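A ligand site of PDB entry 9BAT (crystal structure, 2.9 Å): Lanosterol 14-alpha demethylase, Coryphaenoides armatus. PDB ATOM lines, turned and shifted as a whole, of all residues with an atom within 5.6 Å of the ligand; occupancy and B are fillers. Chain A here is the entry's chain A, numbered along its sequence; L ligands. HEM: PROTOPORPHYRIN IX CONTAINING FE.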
ATOM      1  N   TYR A  78     -18.598  -7.087   2.885  1.00  0.00           N
ATOM      2  CA  TYR A  78     -18.759  -6.576   1.520  1.00  0.00           C
ATOM      3  C   TYR A  78     -19.859  -7.324   0.758  1.00  0.00           C
ATOM      4  O   TYR A  78     -20.073  -7.013  -0.411  1.00  0.00           O
ATOM      5  CB  TYR A  78     -17.446  -6.689   0.741  1.00  0.00           C
ATOM      6  CG  TYR A  78     -16.479  -5.521   0.870  1.00  0.00           C
ATOM      7  CD1 TYR A  78     -16.684  -4.501   1.794  1.00  0.00           C
ATOM      8  CD2 TYR A  78     -15.359  -5.429   0.062  1.00  0.00           C
ATOM      9  CE1 TYR A  78     -15.801  -3.438   1.921  1.00  0.00           C
ATOM     10  CE2 TYR A  78     -14.468  -4.374   0.167  1.00  0.00           C
ATOM     11  CZ  TYR A  78     -14.690  -3.371   1.096  1.00  0.00           C
ATOM     12  OH  TYR A  78     -13.785  -2.355   1.170  1.00  0.00           O
ATOM     13  N   TYR A  92     -20.061 -11.314  -4.351  1.00  0.00           N
ATOM     14  CA  TYR A  92     -19.852 -11.835  -3.018  1.00  0.00           C
ATOM     15  C   TYR A  92     -21.062 -12.606  -2.498  1.00  0.00           C
ATOM     16  O   TYR A  92     -21.333 -12.584  -1.295  1.00  0.00           O
ATOM     17  CB  TYR A  92     -19.529 -10.698  -2.043  1.00  0.00           C
ATOM     18  CG  TYR A  92     -18.184 -10.018  -2.272  1.00  0.00           C
ATOM     19  CD1 TYR A  92     -16.998 -10.659  -1.965  1.00  0.00           C
ATOM     20  CD2 TYR A  92     -18.118  -8.718  -2.775  1.00  0.00           C
ATOM     21  CE1 TYR A  92     -15.771 -10.041  -2.159  1.00  0.00           C
ATOM     22  CE2 TYR A  92     -16.903  -8.088  -2.969  1.00  0.00           C
ATOM     23  CZ  TYR A  92     -15.722  -8.758  -2.657  1.00  0.00           C
ATOM     24  OH  TYR A  92     -14.512  -8.149  -2.840  1.00  0.00           O
ATOM     25  N   PHE A  99     -16.566 -18.107  -6.628  1.00  0.00           N
ATOM     26  CA  PHE A  99     -16.396 -16.676  -6.774  1.00  0.00           C
ATOM     27  C   PHE A  99     -15.122 -16.407  -7.569  1.00  0.00           C
ATOM     28  O   PHE A  99     -15.161 -15.670  -8.552  1.00  0.00           O
ATOM     29  CB  PHE A  99     -16.360 -16.001  -5.391  1.00  0.00           C
ATOM     30  CG  PHE A  99     -16.091 -14.518  -5.411  1.00  0.00           C
ATOM     31  CD1 PHE A  99     -16.861 -13.668  -6.189  1.00  0.00           C
ATOM     32  CD2 PHE A  99     -15.057 -13.980  -4.658  1.00  0.00           C
ATOM     33  CE1 PHE A  99     -16.602 -12.302  -6.203  1.00  0.00           C
ATOM     34  CE2 PHE A  99     -14.807 -12.624  -4.677  1.00  0.00           C
ATOM     35  CZ  PHE A  99     -15.575 -11.781  -5.447  1.00  0.00           C
ATOM     36  N   LYS A 103     -13.913 -14.674 -11.359  1.00  0.00           N
ATOM     37  CA  LYS A 103     -12.896 -13.646 -11.355  1.00  0.00           C
ATOM     38  C   LYS A 103     -11.736 -14.026 -12.262  1.00  0.00           C
ATOM     39  O   LYS A 103     -11.116 -13.157 -12.863  1.00  0.00           O
ATOM     40  CB  LYS A 103     -12.406 -13.372  -9.936  1.00  0.00           C
ATOM     41  CG  LYS A 103     -13.279 -12.427  -9.136  1.00  0.00           C
ATOM     42  CD  LYS A 103     -12.894 -12.342  -7.675  1.00  0.00           C
ATOM     43  CE  LYS A 103     -11.523 -11.716  -7.459  1.00  0.00           C
ATOM     44  NZ  LYS A 103     -11.186 -11.607  -6.020  1.00  0.00           N
ATOM     45  N   LEU A 106     -12.949 -13.301 -15.734  1.00  0.00           N
ATOM     46  CA  LEU A 106     -12.889 -11.886 -16.039  1.00  0.00           C
ATOM     47  C   LEU A 106     -11.462 -11.452 -16.366  1.00  0.00           C
ATOM     48  O   LEU A 106     -11.257 -10.667 -17.287  1.00  0.00           O
ATOM     49  CB  LEU A 106     -13.437 -11.072 -14.875  1.00  0.00           C
ATOM     50  CG  LEU A 106     -14.864 -11.422 -14.425  1.00  0.00           C
ATOM     51  CD1 LEU A 106     -15.256 -10.585 -13.208  1.00  0.00           C
ATOM     52  CD2 LEU A 106     -15.870 -11.222 -15.548  1.00  0.00           C
ATOM     53  N   LEU A 110      -9.502  -9.652 -19.794  1.00  0.00           N
ATOM     54  CA  LEU A 110      -8.887  -8.341 -19.660  1.00  0.00           C
ATOM     55  C   LEU A 110      -7.386  -8.462 -19.852  1.00  0.00           C
ATOM     56  O   LEU A 110      -6.602  -8.338 -18.905  1.00  0.00           O
ATOM     57  CB  LEU A 110      -9.221  -7.773 -18.274  1.00  0.00           C
ATOM     58  CG  LEU A 110     -10.685  -7.387 -18.066  1.00  0.00           C
ATOM     59  CD1 LEU A 110     -10.908  -6.904 -16.655  1.00  0.00           C
ATOM     60  CD2 LEU A 110     -11.102  -6.319 -19.066  1.00  0.00           C
ATOM     61  N   LEU A 157     -16.199  -3.686 -22.683  1.00  0.00           N
ATOM     62  CA  LEU A 157     -16.430  -4.907 -21.918  1.00  0.00           C
ATOM     63  C   LEU A 157     -17.763  -5.571 -22.297  1.00  0.00           C
ATOM     64  O   LEU A 157     -17.879  -6.786 -22.236  1.00  0.00           O
ATOM     65  CB  LEU A 157     -16.389  -4.586 -20.427  1.00  0.00           C
ATOM     66  CG  LEU A 157     -15.188  -3.762 -19.975  1.00  0.00           C
ATOM     67  CD1 LEU A 157     -15.224  -3.471 -18.486  1.00  0.00           C
ATOM     68  CD2 LEU A 157     -13.884  -4.467 -20.360  1.00  0.00           C
ATOM     69  N   GLY A 254     -21.730  -5.837 -13.131  1.00  0.00           N
ATOM     70  CA  GLY A 254     -20.909  -5.584 -11.950  1.00  0.00           C
ATOM     71  C   GLY A 254     -19.519  -5.066 -12.294  1.00  0.00           C
ATOM     72  O   GLY A 254     -18.938  -4.314 -11.510  1.00  0.00           O
ATOM     73  N   LEU A 255     -19.007  -5.443 -13.462  1.00  0.00           N
ATOM     74  CA  LEU A 255     -17.666  -5.027 -13.842  1.00  0.00           C
ATOM     75  C   LEU A 255     -17.644  -3.570 -14.309  1.00  0.00           C
ATOM     76  O   LEU A 255     -16.608  -2.913 -14.188  1.00  0.00           O
ATOM     77  CB  LEU A 255     -17.120  -5.954 -14.938  1.00  0.00           C
ATOM     78  CG  LEU A 255     -15.616  -5.884 -15.168  1.00  0.00           C
ATOM     79  CD1 LEU A 255     -14.861  -6.569 -14.041  1.00  0.00           C
ATOM     80  CD2 LEU A 255     -15.253  -6.526 -16.501  1.00  0.00           C
ATOM     81  N   LEU A 256     -18.762  -3.084 -14.871  1.00  0.00           N
ATOM     82  CA  LEU A 256     -18.851  -1.676 -15.232  1.00  0.00           C
ATOM     83  C   LEU A 256     -19.059  -0.813 -13.979  1.00  0.00           C
ATOM     84  O   LEU A 256     -18.579   0.328 -13.934  1.00  0.00           O
ATOM     85  CB  LEU A 256     -19.995  -1.486 -16.239  1.00  0.00           C
ATOM     86  CG  LEU A 256     -20.198  -0.057 -16.744  1.00  0.00           C
ATOM     87  CD1 LEU A 256     -20.315  -0.018 -18.258  1.00  0.00           C
ATOM     88  CD2 LEU A 256     -21.425   0.569 -16.108  1.00  0.00           C
ATOM     89  N   ALA A 258     -18.035  -1.488 -10.713  1.00  0.00           N
ATOM     90  CA  ALA A 258     -16.857  -1.462  -9.860  1.00  0.00           C
ATOM     91  C   ALA A 258     -15.771  -0.540 -10.429  1.00  0.00           C
ATOM     92  O   ALA A 258     -14.810  -0.247  -9.707  1.00  0.00           O
ATOM     93  CB  ALA A 258     -16.319  -2.855  -9.653  1.00  0.00           C
ATOM     94  N   GLY A 259     -15.898  -0.163 -11.710  1.00  0.00           N
ATOM     95  CA  GLY A 259     -14.914   0.697 -12.359  1.00  0.00           C
ATOM     96  C   GLY A 259     -15.463   2.074 -12.764  1.00  0.00           C
ATOM     97  O   GLY A 259     -14.738   2.916 -13.298  1.00  0.00           O
ATOM     98  N   THR A 262     -14.895   4.819  -9.637  1.00  0.00           N
ATOM     99  CA  THR A 262     -13.436   4.780  -9.406  1.00  0.00           C
ATOM    100  C   THR A 262     -12.750   5.526 -10.540  1.00  0.00           C
ATOM    101  O   THR A 262     -12.051   6.517 -10.269  1.00  0.00           O
ATOM    102  CB  THR A 262     -12.956   3.328  -9.328  1.00  0.00           C
ATOM    103  OG1 THR A 262     -13.393   2.681 -10.525  1.00  0.00           O
ATOM    104  CG2 THR A 262     -13.491   2.594  -8.110  1.00  0.00           C
ATOM    105  N   SER A 263     -12.992   5.089 -11.762  1.00  0.00           N
ATOM    106  CA  SER A 263     -12.318   5.711 -12.932  1.00  0.00           C
ATOM    107  C   SER A 263     -12.787   7.153 -13.096  1.00  0.00           C
ATOM    108  O   SER A 263     -11.934   8.014 -13.322  1.00  0.00           O
ATOM    109  CB  SER A 263     -12.576   4.899 -14.155  1.00  0.00           C
ATOM    110  OG  SER A 263     -12.275   3.529 -13.921  1.00  0.00           O
ATOM    111  N   THR A 266     -11.306   9.672 -10.590  1.00  0.00           N
ATOM    112  CA  THR A 266      -9.851   9.877 -10.774  1.00  0.00           C
ATOM    113  C   THR A 266      -9.630  10.750 -12.013  1.00  0.00           C
ATOM    114  O   THR A 266      -8.822  11.675 -11.943  1.00  0.00           O
ATOM    115  CB  THR A 266      -9.133   8.523 -10.785  1.00  0.00           C
ATOM    116  OG1 THR A 266      -9.515   7.821  -9.609  1.00  0.00           O
ATOM    117  CG2 THR A 266      -7.632   8.668 -10.848  1.00  0.00           C
ATOM    118  N   LEU A 318      -3.950   9.343  -8.152  1.00  0.00           N
ATOM    119  CA  LEU A 318      -4.384   8.196  -7.358  1.00  0.00           C
ATOM    120  C   LEU A 318      -3.741   8.219  -5.970  1.00  0.00           C
ATOM    121  O   LEU A 318      -4.230   7.607  -5.028  1.00  0.00           O
ATOM    122  CB  LEU A 318      -4.047   6.907  -8.106  1.00  0.00           C
ATOM    123  CG  LEU A 318      -4.948   6.571  -9.302  1.00  0.00           C
ATOM    124  CD1 LEU A 318      -4.325   5.489 -10.163  1.00  0.00           C
ATOM    125  CD2 LEU A 318      -6.328   6.138  -8.836  1.00  0.00           C
ATOM    126  N   PRO A 323      -9.950   6.706  -5.069  1.00  0.00           N
ATOM    127  CA  PRO A 323     -11.405   6.642  -5.010  1.00  0.00           C
ATOM    128  C   PRO A 323     -11.927   5.653  -3.967  1.00  0.00           C
ATOM    129  O   PRO A 323     -13.007   5.833  -3.437  1.00  0.00           O
ATOM    130  CB  PRO A 323     -11.833   6.249  -6.429  1.00  0.00           C
ATOM    131  CG  PRO A 323     -10.622   5.529  -6.990  1.00  0.00           C
ATOM    132  CD  PRO A 323      -9.417   6.186  -6.345  1.00  0.00           C
ATOM    133  N   ILE A 324     -11.146   4.607  -3.697  1.00  0.00           N
ATOM    134  CA  ILE A 324     -11.442   3.706  -2.597  1.00  0.00           C
ATOM    135  C   ILE A 324     -10.698   4.246  -1.391  1.00  0.00           C
ATOM    136  O   ILE A 324      -9.465   4.204  -1.332  1.00  0.00           O
ATOM    137  CB  ILE A 324     -11.022   2.256  -2.917  1.00  0.00           C
ATOM    138  CG1 ILE A 324     -11.526   1.805  -4.283  1.00  0.00           C
ATOM    139  CG2 ILE A 324     -11.497   1.328  -1.817  1.00  0.00           C
ATOM    140  CD1 ILE A 324     -12.979   1.448  -4.298  1.00  0.00           C
ATOM    141  N   MET A 327     -10.219  -0.064   2.530  1.00  0.00           N
ATOM    142  CA  MET A 327     -10.521  -1.476   2.383  1.00  0.00           C
ATOM    143  C   MET A 327     -10.772  -2.080   3.761  1.00  0.00           C
ATOM    144  O   MET A 327     -10.028  -1.799   4.693  1.00  0.00           O
ATOM    145  CB  MET A 327      -9.355  -2.192   1.711  1.00  0.00           C
ATOM    146  CG  MET A 327      -9.117  -1.720   0.292  1.00  0.00           C
ATOM    147  SD  MET A 327      -7.581  -2.347  -0.410  1.00  0.00           S
ATOM    148  CE  MET A 327      -7.823  -4.117  -0.252  1.00  0.00           C
ATOM    149  N   MET A 328     -11.824  -2.879   3.880  1.00  0.00           N
ATOM    150  CA  MET A 328     -12.266  -3.386   5.174  1.00  0.00           C
ATOM    151  C   MET A 328     -12.423  -4.907   5.139  1.00  0.00           C
ATOM    152  O   MET A 328     -12.897  -5.478   4.157  1.00  0.00           O
ATOM    153  CB  MET A 328     -13.606  -2.791   5.603  1.00  0.00           C
ATOM    154  CG  MET A 328     -13.637  -1.279   5.679  1.00  0.00           C
ATOM    155  SD  MET A 328     -15.315  -0.733   6.120  1.00  0.00           S
ATOM    156  CE  MET A 328     -15.953  -0.317   4.494  1.00  0.00           C
ATOM    157  N   ARG A 329     -12.046  -5.543   6.259  1.00  0.00           N
ATOM    158  CA  ARG A 329     -12.199  -6.979   6.447  1.00  0.00           C
ATOM    159  C   ARG A 329     -12.658  -7.237   7.874  1.00  0.00           C
ATOM    160  O   ARG A 329     -12.371  -6.466   8.784  1.00  0.00           O
ATOM    161  CB  ARG A 329     -10.885  -7.706   6.194  1.00  0.00           C
ATOM    162  CG  ARG A 329     -10.368  -7.612   4.759  1.00  0.00           C
ATOM    163  CD  ARG A 329     -11.317  -8.275   3.781  1.00  0.00           C
ATOM    164  NE  ARG A 329     -10.773  -8.206   2.435  1.00  0.00           N
ATOM    165  CZ  ARG A 329     -10.803  -7.139   1.663  1.00  0.00           C
ATOM    166  NH1 ARG A 329     -11.364  -6.028   2.089  1.00  0.00           N
ATOM    167  NH2 ARG A 329     -10.304  -7.191   0.442  1.00  0.00           N
ATOM    168  N   VAL A 387      -1.088   2.102  -2.415  1.00  0.00           N
ATOM    169  CA  VAL A 387      -1.992   0.990  -2.697  1.00  0.00           C
ATOM    170  C   VAL A 387      -3.348   1.485  -3.179  1.00  0.00           C
ATOM    171  O   VAL A 387      -4.383   1.062  -2.655  1.00  0.00           O
ATOM    172  CB  VAL A 387      -2.139   0.120  -1.437  1.00  0.00           C
ATOM    173  CG1 VAL A 387      -0.864  -0.656  -1.174  1.00  0.00           C
ATOM    174  CG2 VAL A 387      -2.510   0.944  -0.234  1.00  0.00           C
ATOM    175  N   PRO A 388      -3.425   2.318  -4.246  1.00  0.00           N
ATOM    176  CA  PRO A 388      -4.730   2.757  -4.731  1.00  0.00           C
ATOM    177  C   PRO A 388      -5.589   1.595  -5.211  1.00  0.00           C
ATOM    178  O   PRO A 388      -6.781   1.584  -4.941  1.00  0.00           O
ATOM    179  CB  PRO A 388      -4.401   3.740  -5.855  1.00  0.00           C
ATOM    180  CG  PRO A 388      -3.037   3.318  -6.329  1.00  0.00           C
ATOM    181  CD  PRO A 388      -2.328   2.800  -5.095  1.00  0.00           C
ATOM    182  N   PHE A 389      -4.986   0.628  -5.909  1.00  0.00           N
ATOM    183  CA  PHE A 389      -5.739  -0.495  -6.463  1.00  0.00           C
ATOM    184  C   PHE A 389      -5.684  -1.702  -5.534  1.00  0.00           C
ATOM    185  O   PHE A 389      -6.063  -2.802  -5.927  1.00  0.00           O
ATOM    186  CB  PHE A 389      -5.162  -0.908  -7.812  1.00  0.00           C
ATOM    187  CG  PHE A 389      -5.355   0.085  -8.922  1.00  0.00           C
ATOM    188  CD1 PHE A 389      -6.513   0.086  -9.659  1.00  0.00           C
ATOM    189  CD2 PHE A 389      -4.369   1.012  -9.222  1.00  0.00           C
ATOM    190  CE1 PHE A 389      -6.700   0.973 -10.709  1.00  0.00           C
ATOM    191  CE2 PHE A 389      -4.555   1.909 -10.253  1.00  0.00           C
ATOM    192  CZ  PHE A 389      -5.712   1.894 -11.001  1.00  0.00           C
ATOM    193  N   GLY A 390      -5.206  -1.502  -4.303  1.00  0.00           N
ATOM    194  CA  GLY A 390      -4.939  -2.598  -3.399  1.00  0.00           C
ATOM    195  C   GLY A 390      -3.525  -3.103  -3.605  1.00  0.00           C
ATOM    196  O   GLY A 390      -2.711  -2.406  -4.203  1.00  0.00           O
ATOM    197  N   HIS A 394      -5.100  -9.052  -2.581  1.00  0.00           N
ATOM    198  CA  HIS A 394      -6.356  -8.326  -2.758  1.00  0.00           C
ATOM    199  C   HIS A 394      -6.065  -7.115  -3.621  1.00  0.00           C
ATOM    200  O   HIS A 394      -5.571  -6.121  -3.107  1.00  0.00           O
ATOM    201  CB  HIS A 394      -6.961  -7.975  -1.396  1.00  0.00           C
ATOM    202  CG  HIS A 394      -6.895  -9.108  -0.430  1.00  0.00           C
ATOM    203  ND1 HIS A 394      -7.902 -10.035  -0.301  1.00  0.00           N
ATOM    204  CD2 HIS A 394      -5.933  -9.497   0.404  1.00  0.00           C
ATOM    205  CE1 HIS A 394      -7.567 -10.926   0.621  1.00  0.00           C
ATOM    206  NE2 HIS A 394      -6.369 -10.615   1.057  1.00  0.00           N
ATOM    207  N   ARG A 395      -6.374  -7.219  -4.913  1.00  0.00           N
ATOM    208  CA  ARG A 395      -5.979  -6.215  -5.888  1.00  0.00           C
ATOM    209  C   ARG A 395      -7.049  -6.069  -6.945  1.00  0.00           C
ATOM    210  O   ARG A 395      -7.752  -7.016  -7.260  1.00  0.00           O
ATOM    211  CB  ARG A 395      -4.647  -6.623  -6.520  1.00  0.00           C
ATOM    212  CG  ARG A 395      -3.935  -5.492  -7.245  1.00  0.00           C
ATOM    213  CD  ARG A 395      -2.479  -5.845  -7.465  1.00  0.00           C
ATOM    214  NE  ARG A 395      -1.758  -4.720  -8.046  1.00  0.00           N
ATOM    215  CZ  ARG A 395      -0.667  -4.819  -8.784  1.00  0.00           C
ATOM    216  NH1 ARG A 395      -0.119  -6.005  -9.009  1.00  0.00           N
ATOM    217  NH2 ARG A 395      -0.127  -3.736  -9.312  1.00  0.00           N
ATOM    218  N   CYS A 396      -7.168  -4.854  -7.488  1.00  0.00           N
ATOM    219  CA  CYS A 396      -8.128  -4.585  -8.548  1.00  0.00           C
ATOM    220  C   CYS A 396      -7.735  -5.349  -9.813  1.00  0.00           C
ATOM    221  O   CYS A 396      -6.622  -5.227 -10.309  1.00  0.00           O
ATOM    222  CB  CYS A 396      -8.173  -3.094  -8.848  1.00  0.00           C
ATOM    223  SG  CYS A 396      -9.564  -2.572  -9.892  1.00  0.00           S
ATOM    224  N   ILE A 397      -8.691  -6.115 -10.349  1.00  0.00           N
ATOM    225  CA  ILE A 397      -8.463  -6.809 -11.610  1.00  0.00           C
ATOM    226  C   ILE A 397      -8.656  -5.871 -12.798  1.00  0.00           C
ATOM    227  O   ILE A 397      -8.122  -6.136 -13.879  1.00  0.00           O
ATOM    228  CB  ILE A 397      -9.352  -8.052 -11.713  1.00  0.00           C
ATOM    229  CG1 ILE A 397     -10.824  -7.660 -11.800  1.00  0.00           C
ATOM    230  CG2 ILE A 397      -9.100  -9.007 -10.565  1.00  0.00           C
ATOM    231  CD1 ILE A 397     -11.737  -8.847 -11.932  1.00  0.00           C
ATOM    232  N   GLY A 398      -9.387  -4.777 -12.605  1.00  0.00           N
ATOM    233  CA  GLY A 398      -9.544  -3.740 -13.618  1.00  0.00           C
ATOM    234  C   GLY A 398      -8.371  -2.758 -13.737  1.00  0.00           C
ATOM    235  O   GLY A 398      -8.421  -1.838 -14.547  1.00  0.00           O
ATOM    236  N   GLU A 399      -7.299  -2.945 -12.961  1.00  0.00           N
ATOM    237  CA  GLU A 399      -6.198  -1.998 -12.974  1.00  0.00           C
ATOM    238  C   GLU A 399      -5.644  -1.797 -14.379  1.00  0.00           C
ATOM    239  O   GLU A 399      -5.338  -0.682 -14.773  1.00  0.00           O
ATOM    240  CB  GLU A 399      -5.105  -2.459 -12.011  1.00  0.00           C
ATOM    241  CG  GLU A 399      -3.899  -1.539 -11.957  1.00  0.00           C
ATOM    242  CD  GLU A 399      -2.899  -1.899 -10.872  1.00  0.00           C
ATOM    243  OE1 GLU A 399      -3.188  -2.838 -10.090  1.00  0.00           O
ATOM    244  OE2 GLU A 399      -1.839  -1.255 -10.815  1.00  0.00           O
ATOM    245  N   PHE A 401      -7.148  -2.363 -17.335  1.00  0.00           N
ATOM    246  CA  PHE A 401      -8.150  -1.646 -18.112  1.00  0.00           C
ATOM    247  C   PHE A 401      -8.236  -0.192 -17.660  1.00  0.00           C
ATOM    248  O   PHE A 401      -8.485   0.697 -18.467  1.00  0.00           O
ATOM    249  CB  PHE A 401      -9.507  -2.336 -17.987  1.00  0.00           C
ATOM    250  CG  PHE A 401     -10.622  -1.667 -18.745  1.00  0.00           C
ATOM    251  CD1 PHE A 401     -10.675  -1.720 -20.128  1.00  0.00           C
ATOM    252  CD2 PHE A 401     -11.596  -0.943 -18.079  1.00  0.00           C
ATOM    253  CE1 PHE A 401     -11.691  -1.094 -20.817  1.00  0.00           C
ATOM    254  CE2 PHE A 401     -12.631  -0.329 -18.770  1.00  0.00           C
ATOM    255  CZ  PHE A 401     -12.670  -0.400 -20.145  1.00  0.00           C
ATOM    256  N   ALA A 402      -8.052   0.051 -16.350  1.00  0.00           N
ATOM    257  CA  ALA A 402      -8.127   1.397 -15.803  1.00  0.00           C
ATOM    258  C   ALA A 402      -7.054   2.294 -16.423  1.00  0.00           C
ATOM    259  O   ALA A 402      -7.360   3.329 -16.997  1.00  0.00           O
ATOM    260  CB  ALA A 402      -7.990   1.354 -14.297  1.00  0.00           C
ATOM    261  N   GLN A 405      -7.895   2.832 -20.124  1.00  0.00           N
ATOM    262  CA  GLN A 405      -9.041   3.706 -20.286  1.00  0.00           C
ATOM    263  C   GLN A 405      -8.696   5.153 -19.912  1.00  0.00           C
ATOM    264  O   GLN A 405      -9.003   6.068 -20.660  1.00  0.00           O
ATOM    265  CB  GLN A 405     -10.206   3.204 -19.434  1.00  0.00           C
ATOM    266  CG  GLN A 405     -11.484   4.016 -19.595  1.00  0.00           C
ATOM    267  CD  GLN A 405     -12.615   3.500 -18.736  1.00  0.00           C
ATOM    268  OE1 GLN A 405     -13.761   3.406 -19.192  1.00  0.00           O
ATOM    269  NE2 GLN A 405     -12.310   3.197 -17.485  1.00  0.00           N
ATOM    270  N   LEU A 406      -8.071   5.351 -18.745  1.00  0.00           N
ATOM    271  CA  LEU A 406      -7.832   6.688 -18.234  1.00  0.00           C
ATOM    272  C   LEU A 406      -6.837   7.428 -19.124  1.00  0.00           C
ATOM    273  O   LEU A 406      -7.072   8.586 -19.451  1.00  0.00           O
ATOM    274  CB  LEU A 406      -7.319   6.613 -16.796  1.00  0.00           C
ATOM    275  CG  LEU A 406      -8.331   6.140 -15.747  1.00  0.00           C
ATOM    276  CD1 LEU A 406      -7.679   6.047 -14.370  1.00  0.00           C
ATOM    277  CD2 LEU A 406      -9.547   7.039 -15.698  1.00  0.00           C
HETATM  278  CHA HEM L   1     -11.501  -4.422  -6.682  1.00  0.00           C
HETATM  279  CHB HEM L   1      -9.658   0.074  -6.808  1.00  0.00           C
HETATM  280  CHC HEM L   1     -11.054   0.527 -11.448  1.00  0.00           C
HETATM  281  CHD HEM L   1     -13.252  -3.753 -11.165  1.00  0.00           C
HETATM  282  C1A HEM L   1     -10.846  -3.256  -6.349  1.00  0.00           C
HETATM  283  C2A HEM L   1     -10.132  -3.062  -5.133  1.00  0.00           C
HETATM  284  C3A HEM L   1      -9.623  -1.789  -5.163  1.00  0.00           C
HETATM  285  C4A HEM L   1     -10.008  -1.193  -6.398  1.00  0.00           C
HETATM  286  CMA HEM L   1      -8.779  -1.134  -4.051  1.00  0.00           C
HETATM  287  CAA HEM L   1      -9.938  -4.035  -3.983  1.00  0.00           C
HETATM  288  CBA HEM L   1     -11.011  -3.854  -2.914  1.00  0.00           C
HETATM  289  CGA HEM L   1     -10.815  -4.861  -1.802  1.00  0.00           C
HETATM  290  O1A HEM L   1     -11.387  -4.651  -0.700  1.00  0.00           O
HETATM  291  O2A HEM L   1     -10.086  -5.883  -1.992  1.00  0.00           O
HETATM  292  C1B HEM L   1      -9.869   0.572  -8.094  1.00  0.00           C
HETATM  293  C2B HEM L   1      -9.338   1.825  -8.547  1.00  0.00           C
HETATM  294  C3B HEM L   1      -9.728   1.985  -9.868  1.00  0.00           C
HETATM  295  C4B HEM L   1     -10.502   0.747 -10.185  1.00  0.00           C
HETATM  296  CMB HEM L   1      -8.501   2.786  -7.715  1.00  0.00           C
HETATM  297  CAB HEM L   1      -9.497   3.083 -10.872  1.00  0.00           C
HETATM  298  CBB HEM L   1      -8.817   4.179 -10.608  1.00  0.00           C
HETATM  299  C1C HEM L   1     -11.749  -0.608 -11.811  1.00  0.00           C
HETATM  300  C2C HEM L   1     -12.130  -0.962 -13.127  1.00  0.00           C
HETATM  301  C3C HEM L   1     -12.764  -2.197 -13.062  1.00  0.00           C
HETATM  302  C4C HEM L   1     -12.758  -2.566 -11.669  1.00  0.00           C
HETATM  303  CMC HEM L   1     -11.852  -0.122 -14.366  1.00  0.00           C
HETATM  304  CAC HEM L   1     -13.350  -3.023 -14.150  1.00  0.00           C
HETATM  305  CBC HEM L   1     -13.272  -2.777 -15.451  1.00  0.00           C
HETATM  306  C1D HEM L   1     -12.899  -4.281  -9.924  1.00  0.00           C
HETATM  307  C2D HEM L   1     -13.319  -5.640  -9.550  1.00  0.00           C
HETATM  308  C3D HEM L   1     -12.846  -5.861  -8.307  1.00  0.00           C
HETATM  309  C4D HEM L   1     -12.129  -4.602  -7.923  1.00  0.00           C
HETATM  310  CMD HEM L   1     -14.126  -6.645 -10.371  1.00  0.00           C
HETATM  311  CAD HEM L   1     -13.063  -7.187  -7.584  1.00  0.00           C
HETATM  312  CBD HEM L   1     -13.442  -7.100  -6.092  1.00  0.00           C
HETATM  313  CGD HEM L   1     -12.814  -8.312  -5.413  1.00  0.00           C
HETATM  314  O1D HEM L   1     -11.585  -8.510  -5.514  1.00  0.00           O
HETATM  315  O2D HEM L   1     -13.506  -9.154  -4.774  1.00  0.00           O
HETATM  316  NA  HEM L   1     -10.760  -2.085  -7.113  1.00  0.00           N
HETATM  317  NB  HEM L   1     -10.524  -0.029  -9.089  1.00  0.00           N
HETATM  318  NC  HEM L   1     -12.122  -1.577 -10.930  1.00  0.00           N
HETATM  319  ND  HEM L   1     -12.195  -3.680  -8.941  1.00  0.00           N
HETATM  320 FE   HEM L   1     -11.479  -1.882  -8.948  1.00  0.00          FE
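The side-chain amino group (NZ) of Lys 103 lies within salt-bridge range of an oxygen (O1D) of the ligand. The side-chain sulfur (SG) of Cys 396 binds an iron atom (FE) of the ligand, 2.2 Å away. NH2 of Arg 329 lies within salt-bridge range of O2A of the ligand. An oxygen (O2D) of the ligand sits at hydrogen-bond distance from the side-chain hydroxyl (OH) of Tyr 92.
The side-chain hydroxyl (OH) of Tyr 78 is in hydrogen-bond range of the backbone NH (N) of Met 328 (3.4 Å). O of Gly 259 sits at hydrogen-bond distance from OG1 of Thr 262, at 3.1 Å. The backbone NH (N) of Cys 396 lies within hydrogen-bond range of the backbone carbonyl oxygen (O) of Phe 389, at 2.8 Å. The side-chain hydroxyl (OG1) of Thr 262 lies within hydrogen-bond range of the backbone carbonyl oxygen (O) of Ala 258, at 3.4 Å. The backbone carbonyl oxygen of Gly 259 sits at hydrogen-bond distance from the side-chain hydroxyl of Ser 263, at 2.6 Å. The side-chain sulfur (SG) of Cys 396 lies close to the backbone NH (N) of Gly 398, 3.5 Å away. The backbone carbonyl oxygen (O) of Thr 262 sits at hydrogen-bond distance from the side-chain hydroxyl (OG1) of Thr 266 (2.9 Å).
NC of the ligand lies close to O of Ala 258, at 3.2 Å. Residues that only touch the ligand: Tyr 78 (3.2 Å), Phe 99 (3.4 Å), Leu 157 (3.7 Å), Leu 255 (3.3 Å), Gly 259 (3.3 Å), Thr 262 (3.3 Å), Ser 263 (3.7 Å), Thr 266 (3.8 Å), Leu 318 (3.6 Å), Pro 323 (3.5 Å), Ile 324 (3.6 Å), Met 327 (3.4 Å), Pro 388 (3.5 Å), Phe 389 (3.3 Å), Gly 390 (3.6 Å), His 394 (3.8 Å), Ile 397 (3.6 Å), Gly 398 (3.6 Å) and Phe 401 (3.6 Å). Hydrophobic or aromatic side chains within 4 Å of the ligand: Tyr 78, Tyr 92, Phe 99, Leu 157, Leu 255, Ala 258, Leu 318, Pro 323, Ile 324, Met 327, Phe 389, His 394, Ile 397 and Phe 401. 24 residues have an atom within 4 Å of the ligand: Tyr 78, Tyr 92, Phe 99, Lys 103, Leu 157, Leu 255, Ala 258, Gly 259, Thr 262, Ser 263, Thr 266, Leu 318, Pro 323, Ile 324, Met 327, Arg 329, Pro 388, Phe 389, Gly 390, His 394, Cys 396, Ile 397, Gly 398 and Phe 401.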
